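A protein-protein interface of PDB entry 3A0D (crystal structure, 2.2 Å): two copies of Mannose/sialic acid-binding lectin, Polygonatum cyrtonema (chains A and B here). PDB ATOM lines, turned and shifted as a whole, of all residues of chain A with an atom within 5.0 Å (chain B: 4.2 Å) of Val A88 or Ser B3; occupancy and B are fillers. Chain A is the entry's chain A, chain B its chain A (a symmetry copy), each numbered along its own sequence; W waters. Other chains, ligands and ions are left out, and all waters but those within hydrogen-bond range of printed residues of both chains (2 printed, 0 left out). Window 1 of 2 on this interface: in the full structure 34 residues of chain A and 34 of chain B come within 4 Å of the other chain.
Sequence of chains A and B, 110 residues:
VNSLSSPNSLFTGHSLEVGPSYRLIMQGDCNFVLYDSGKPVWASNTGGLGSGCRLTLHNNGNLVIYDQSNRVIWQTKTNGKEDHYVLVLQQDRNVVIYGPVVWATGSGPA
Asn A2 touches its own counterpart, Asn B2. Asn A2 touches Ser B3, and with the chains exchanged Ser A3 touches Asn B2. Ser A3 touches Val B88, and with the chains exchanged Val A88 touches Ser B3. Val B86 touches its own counterpart, Val A86. 5 positions are printed for both chains. Of the 10 pairs that touch across the chains among the printed residues, 6 have their exchanged pair printed and touching as well.
Water W1 lies within hydrogen-bond range of NE2 of Gln A91 (2.6 Å) and O of Ser B3 (2.7 Å). Water W2 lies within hydrogen-bond range of OG of Ser B3 (2.8 Å) and OE1 of Gln A91 (2.9 Å).
Hydrophobic or aromatic side chains of chain A that line the printed part of chain B: Val A86, Val A88 and Tyr A98.
Of chain B, only Ser B3 (3.6 Å) comes within 4 Å of Val A88. Of chain A, only Asn A2 (2.7 Å), Val A88 (3.6 Å) and Gln A91 (3.7 Å) come within 4 Å of Ser B3. Of the printed residues of chain B, Val A86 touches Val B86. Printed residues of chain B within 4 Å of Asn A2: Val B1 (3.5 Å), Asn B2 (2.4 Å) and Ser B3 (2.7 Å). Printed residues of chain A within 4 Å of Val B1: Asn A2 and Gln A91. The nearest printed residue of chain A that does not touch Asn B2 is Gln A91 (6.4 Å).
N of Leu A89 sits at hydrogen-bond distance from O of Asn A2. The backbone NH of Tyr A98 is in hydrogen-bond range of the backbone carbonyl oxygen of Val A86, 2.9 Å away. The backbone NH of Val A88 is in hydrogen-bond range of the backbone carbonyl oxygen of Val A96, at 2.7 Å. OE1 of Gln A90 lies within hydrogen-bond range of OH of Tyr A98, 2.5 Å away.
The side-chain amide oxygen (OD1) of Asn B2 is in hydrogen-bond range of the backbone NH (N) of Asn A2, 2.8 Å away. ND2 of Asn A2 sits at hydrogen-bond distance from OG of Ser B3 (2.7 Å). OG of Ser A3 lies within hydrogen-bond range of ND2 of Asn B2, at 2.7 Å.
Val B1 touches Asn A2. CG1 of Val B88 touches OG of Ser A3, 3.6 Å away. Val A86 touches Val B86 (CG1 to CG1, 3.7 Å). OG of Ser B3 touches CG1 of Val A88 (3.6 Å). NE2 of Gln A91 touches CG2 of Val B1, at 3.4 Å. O of Ser B3 touches NE2 of Gln A91, at 3.7 Å. Val B86 touches Tyr A98 (CG1 to CD1, 3.5 Å).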
ATOM      1  N   ASN A   2      20.933  -1.753  -3.051  1.00  0.00           N
ATOM      2  CA  ASN A   2      19.622  -1.798  -2.410  1.00  0.00           C
ATOM      3  C   ASN A   2      19.593  -2.731  -1.200  1.00  0.00           C
ATOM      4  O   ASN A   2      18.528  -3.181  -0.784  1.00  0.00           O
ATOM      5  CB  ASN A   2      18.535  -2.211  -3.411  1.00  0.00           C
ATOM      6  CG  ASN A   2      18.782  -3.575  -4.020  1.00  0.00           C
ATOM      7  OD1 ASN A   2      19.752  -3.775  -4.744  1.00  0.00           O
ATOM      8  ND2 ASN A   2      17.901  -4.522  -3.729  1.00  0.00           N
ATOM      9  N   SER A   3      20.764  -3.003  -0.629  1.00  0.00           N
ATOM     10  CA  SER A   3      20.850  -3.877   0.535  1.00  0.00           C
ATOM     11  C   SER A   3      21.917  -3.437   1.534  1.00  0.00           C
ATOM     12  O   SER A   3      22.882  -2.757   1.181  1.00  0.00           O
ATOM     13  CB  SER A   3      21.148  -5.314   0.101  1.00  0.00           C
ATOM     14  OG  SER A   3      22.426  -5.405  -0.511  1.00  0.00           O
ATOM     15  N   VAL A  86      20.653  -9.621   6.403  1.00  0.00           N
ATOM     16  CA  VAL A  86      20.652  -8.587   5.382  1.00  0.00           C
ATOM     17  C   VAL A  86      19.327  -7.830   5.399  1.00  0.00           C
ATOM     18  O   VAL A  86      18.275  -8.406   5.694  1.00  0.00           O
ATOM     19  CB  VAL A  86      20.869  -9.193   3.968  1.00  0.00           C
ATOM     20  CG1 VAL A  86      19.626  -9.953   3.527  1.00  0.00           C
ATOM     21  CG2 VAL A  86      21.216  -8.097   2.971  1.00  0.00           C
ATOM     22  N   LEU A  87      19.403  -6.535   5.110  1.00  0.00           N
ATOM     23  CA  LEU A  87      18.236  -5.665   5.036  1.00  0.00           C
ATOM     24  C   LEU A  87      18.120  -5.343   3.552  1.00  0.00           C
ATOM     25  O   LEU A  87      19.098  -4.936   2.930  1.00  0.00           O
ATOM     26  CB  LEU A  87      18.467  -4.372   5.817  1.00  0.00           C
ATOM     27  CG  LEU A  87      17.377  -3.320   5.592  1.00  0.00           C
ATOM     28  CD1 LEU A  87      16.059  -3.815   6.186  1.00  0.00           C
ATOM     29  CD2 LEU A  87      17.797  -2.002   6.213  1.00  0.00           C
ATOM     30  N   VAL A  88      16.934  -5.508   2.983  1.00  0.00           N
ATOM     31  CA  VAL A  88      16.773  -5.269   1.556  1.00  0.00           C
ATOM     32  C   VAL A  88      15.568  -4.430   1.142  1.00  0.00           C
ATOM     33  O   VAL A  88      14.454  -4.648   1.616  1.00  0.00           O
ATOM     34  CB  VAL A  88      16.681  -6.621   0.804  1.00  0.00           C
ATOM     35  CG1 VAL A  88      16.545  -6.388  -0.684  1.00  0.00           C
ATOM     36  CG2 VAL A  88      17.911  -7.466   1.101  1.00  0.00           C
ATOM     37  N   LEU A  89      15.811  -3.465   0.261  1.00  0.00           N
ATOM     38  CA  LEU A  89      14.750  -2.633  -0.304  1.00  0.00           C
ATOM     39  C   LEU A  89      14.478  -3.359  -1.620  1.00  0.00           C
ATOM     40  O   LEU A  89      15.306  -3.335  -2.528  1.00  0.00           O
ATOM     41  CB  LEU A  89      15.244  -1.216  -0.593  1.00  0.00           C
ATOM     42  CG  LEU A  89      14.382  -0.415  -1.576  1.00  0.00           C
ATOM     43  CD1 LEU A  89      12.945  -0.311  -1.058  1.00  0.00           C
ATOM     44  CD2 LEU A  89      14.988   0.968  -1.773  1.00  0.00           C
ATOM     45  N   GLN A  90      13.328  -4.010  -1.712  1.00  0.00           N
ATOM     46  CA  GLN A  90      12.985  -4.794  -2.890  1.00  0.00           C
ATOM     47  C   GLN A  90      12.294  -4.047  -4.022  1.00  0.00           C
ATOM     48  O   GLN A  90      11.701  -2.984  -3.820  1.00  0.00           O
ATOM     49  CB  GLN A  90      12.130  -5.986  -2.458  1.00  0.00           C
ATOM     50  CG  GLN A  90      12.829  -6.870  -1.430  1.00  0.00           C
ATOM     51  CD  GLN A  90      12.018  -8.090  -1.028  1.00  0.00           C
ATOM     52  OE1 GLN A  90      12.570  -9.066  -0.523  1.00  0.00           O
ATOM     53  NE2 GLN A  90      10.705  -8.036  -1.239  1.00  0.00           N
ATOM     54  N   GLN A  91      12.376  -4.610  -5.223  1.00  0.00           N
ATOM     55  CA  GLN A  91      11.734  -3.993  -6.373  1.00  0.00           C
ATOM     56  C   GLN A  91      10.221  -4.013  -6.212  1.00  0.00           C
ATOM     57  O   GLN A  91       9.521  -3.280  -6.903  1.00  0.00           O
ATOM     58  CB  GLN A  91      12.141  -4.683  -7.680  1.00  0.00           C
ATOM     59  CG  GLN A  91      12.533  -6.131  -7.555  1.00  0.00           C
ATOM     60  CD  GLN A  91      13.864  -6.309  -6.857  1.00  0.00           C
ATOM     61  OE1 GLN A  91      13.956  -6.218  -5.633  1.00  0.00           O
ATOM     62  NE2 GLN A  91      14.910  -6.555  -7.639  1.00  0.00           N
ATOM     63  N   ASN A  94       8.863  -3.602  -0.922  1.00  0.00           N
ATOM     64  CA  ASN A  94       8.841  -4.033   0.468  1.00  0.00           C
ATOM     65  C   ASN A  94      10.278  -3.908   0.977  1.00  0.00           C
ATOM     66  O   ASN A  94      11.221  -4.005   0.191  1.00  0.00           O
ATOM     67  CB  ASN A  94       8.367  -5.485   0.566  1.00  0.00           C
ATOM     68  CG  ASN A  94       7.786  -5.823   1.932  1.00  0.00           C
ATOM     69  OD1 ASN A  94       7.740  -4.978   2.823  1.00  0.00           O
ATOM     70  ND2 ASN A  94       7.335  -7.063   2.096  1.00  0.00           N
ATOM     71  N   VAL A  95      10.439  -3.652   2.273  1.00  0.00           N
ATOM     72  CA  VAL A  95      11.758  -3.537   2.898  1.00  0.00           C
ATOM     73  C   VAL A  95      11.792  -4.708   3.868  1.00  0.00           C
ATOM     74  O   VAL A  95      10.971  -4.792   4.783  1.00  0.00           O
ATOM     75  CB  VAL A  95      11.922  -2.195   3.651  1.00  0.00           C
ATOM     76  CG1 VAL A  95      13.238  -2.176   4.416  1.00  0.00           C
ATOM     77  CG2 VAL A  95      11.895  -1.037   2.651  1.00  0.00           C
ATOM     78  N   VAL A  96      12.749  -5.608   3.676  1.00  0.00           N
ATOM     79  CA  VAL A  96      12.803  -6.819   4.478  1.00  0.00           C
ATOM     80  C   VAL A  96      14.149  -7.225   5.060  1.00  0.00           C
ATOM     81  O   VAL A  96      15.192  -7.031   4.445  1.00  0.00           O
ATOM     82  CB  VAL A  96      12.298  -8.008   3.623  1.00  0.00           C
ATOM     83  CG1 VAL A  96      12.092  -9.246   4.492  1.00  0.00           C
ATOM     84  CG2 VAL A  96      11.026  -7.613   2.893  1.00  0.00           C
ATOM     85  N   ILE A  97      14.102  -7.802   6.256  1.00  0.00           N
ATOM     86  CA  ILE A  97      15.295  -8.313   6.916  1.00  0.00           C
ATOM     87  C   ILE A  97      15.234  -9.831   6.748  1.00  0.00           C
ATOM     88  O   ILE A  97      14.241 -10.459   7.126  1.00  0.00           O
ATOM     89  CB  ILE A  97      15.313  -8.001   8.430  1.00  0.00           C
ATOM     90  CG1 ILE A  97      15.418  -6.491   8.661  1.00  0.00           C
ATOM     91  CG2 ILE A  97      16.493  -8.713   9.091  1.00  0.00           C
ATOM     92  CD1 ILE A  97      15.423  -6.098  10.129  1.00  0.00           C
ATOM     93  N   TYR A  98      16.276 -10.413   6.162  1.00  0.00           N
ATOM     94  CA  TYR A  98      16.337 -11.861   5.962  1.00  0.00           C
ATOM     95  C   TYR A  98      17.533 -12.442   6.697  1.00  0.00           C
ATOM     96  O   TYR A  98      18.559 -11.785   6.841  1.00  0.00           O
ATOM     97  CB  TYR A  98      16.497 -12.225   4.485  1.00  0.00           C
ATOM     98  CG  TYR A  98      15.332 -11.898   3.591  1.00  0.00           C
ATOM     99  CD1 TYR A  98      15.267 -10.677   2.920  1.00  0.00           C
ATOM    100  CD2 TYR A  98      14.333 -12.839   3.350  1.00  0.00           C
ATOM    101  CE1 TYR A  98      14.239 -10.407   2.022  1.00  0.00           C
ATOM    102  CE2 TYR A  98      13.300 -12.577   2.454  1.00  0.00           C
ATOM    103  CZ  TYR A  98      13.263 -11.360   1.793  1.00  0.00           C
ATOM    104  OH  TYR A  98      12.251 -11.098   0.899  1.00  0.00           O
ATOM    105  N   VAL B   1      20.376  -3.058  -9.406  1.00  0.00           N
ATOM    106  CA  VAL B   1      19.907  -3.867  -8.251  1.00  0.00           C
ATOM    107  C   VAL B   1      20.966  -4.925  -7.947  1.00  0.00           C
ATOM    108  O   VAL B   1      21.632  -5.411  -8.862  1.00  0.00           O
ATOM    109  CB  VAL B   1      18.548  -4.548  -8.578  1.00  0.00           C
ATOM    110  CG1 VAL B   1      18.700  -5.454  -9.789  1.00  0.00           C
ATOM    111  CG2 VAL B   1      18.044  -5.341  -7.384  1.00  0.00           C
ATOM    112  N   ASN B   2      21.145  -5.260  -6.672  1.00  0.00           N
ATOM    113  CA  ASN B   2      22.129  -6.274  -6.305  1.00  0.00           C
ATOM    114  C   ASN B   2      21.513  -7.435  -5.525  1.00  0.00           C
ATOM    115  O   ASN B   2      22.216  -8.160  -4.824  1.00  0.00           O
ATOM    116  CB  ASN B   2      23.279  -5.658  -5.498  1.00  0.00           C
ATOM    117  CG  ASN B   2      22.814  -5.004  -4.215  1.00  0.00           C
ATOM    118  OD1 ASN B   2      22.086  -4.015  -4.240  1.00  0.00           O
ATOM    119  ND2 ASN B   2      23.233  -5.553  -3.083  1.00  0.00           N
ATOM    120  N   SER B   3      20.202  -7.617  -5.664  1.00  0.00           N
ATOM    121  CA  SER B   3      19.513  -8.699  -4.970  1.00  0.00           C
ATOM    122  C   SER B   3      18.391  -9.319  -5.796  1.00  0.00           C
ATOM    123  O   SER B   3      17.831  -8.685  -6.692  1.00  0.00           O
ATOM    124  CB  SER B   3      18.928  -8.194  -3.648  1.00  0.00           C
ATOM    125  OG  SER B   3      17.922  -7.218  -3.878  1.00  0.00           O
ATOM    126  N   LEU B   4      18.079 -10.573  -5.481  1.00  0.00           N
ATOM    127  CA  LEU B   4      17.011 -11.310  -6.136  1.00  0.00           C
ATOM    128  C   LEU B   4      16.220 -11.973  -5.018  1.00  0.00           C
ATOM    129  O   LEU B   4      16.761 -12.772  -4.252  1.00  0.00           O
ATOM    130  CB  LEU B   4      17.571 -12.386  -7.072  1.00  0.00           C
ATOM    131  CG  LEU B   4      16.522 -13.315  -7.706  1.00  0.00           C
ATOM    132  CD1 LEU B   4      15.647 -12.536  -8.693  1.00  0.00           C
ATOM    133  CD2 LEU B   4      17.223 -14.451  -8.425  1.00  0.00           C
ATOM    134  N   LEU B  16      23.035  -8.967 -11.378  1.00  0.00           N
ATOM    135  CA  LEU B  16      22.965  -8.188 -10.157  1.00  0.00           C
ATOM    136  C   LEU B  16      24.278  -7.421 -10.189  1.00  0.00           C
ATOM    137  O   LEU B  16      25.288  -7.937 -10.670  1.00  0.00           O
ATOM    138  CB  LEU B  16      22.903  -9.106  -8.931  1.00  0.00           C
ATOM    139  CG  LEU B  16      21.726 -10.088  -8.872  1.00  0.00           C
ATOM    140  CD1 LEU B  16      21.720 -10.790  -7.523  1.00  0.00           C
ATOM    141  CD2 LEU B  16      20.411  -9.346  -9.082  1.00  0.00           C
ATOM    142  N   VAL B  86      16.199 -14.343  -0.008  1.00  0.00           N
ATOM    143  CA  VAL B  86      16.818 -13.373  -0.894  1.00  0.00           C
ATOM    144  C   VAL B  86      18.246 -13.797  -1.227  1.00  0.00           C
ATOM    145  O   VAL B  86      18.934 -14.402  -0.399  1.00  0.00           O
ATOM    146  CB  VAL B  86      16.850 -11.961  -0.247  1.00  0.00           C
ATOM    147  CG1 VAL B  86      17.869 -11.925   0.883  1.00  0.00           C
ATOM    148  CG2 VAL B  86      17.166 -10.905  -1.295  1.00  0.00           C
ATOM    149  N   LEU B  87      18.661 -13.498  -2.454  1.00  0.00           N
ATOM    150  CA  LEU B  87      20.008 -13.787  -2.932  1.00  0.00           C
ATOM    151  C   LEU B  87      20.647 -12.411  -3.063  1.00  0.00           C
ATOM    152  O   LEU B  87      20.070 -11.517  -3.678  1.00  0.00           O
ATOM    153  CB  LEU B  87      19.968 -14.458  -4.304  1.00  0.00           C
ATOM    154  CG  LEU B  87      21.345 -14.579  -4.964  1.00  0.00           C
ATOM    155  CD1 LEU B  87      22.211 -15.552  -4.164  1.00  0.00           C
ATOM    156  CD2 LEU B  87      21.190 -15.040  -6.400  1.00  0.00           C
ATOM    157  N   VAL B  88      21.836 -12.236  -2.503  1.00  0.00           N
ATOM    158  CA  VAL B  88      22.474 -10.928  -2.547  1.00  0.00           C
ATOM    159  C   VAL B  88      23.945 -10.905  -2.952  1.00  0.00           C
ATOM    160  O   VAL B  88      24.747 -11.700  -2.463  1.00  0.00           O
ATOM    161  CB  VAL B  88      22.361 -10.241  -1.163  1.00  0.00           C
ATOM    162  CG1 VAL B  88      22.993  -8.867  -1.201  1.00  0.00           C
ATOM    163  CG2 VAL B  88      20.900 -10.145  -0.748  1.00  0.00           C
HETATM  164  O   HOH W   1      16.055  -8.579  -8.724  1.00  0.00           O
HETATM  165  O   HOH W   2      15.419  -8.334  -4.254  1.00  0.00           O
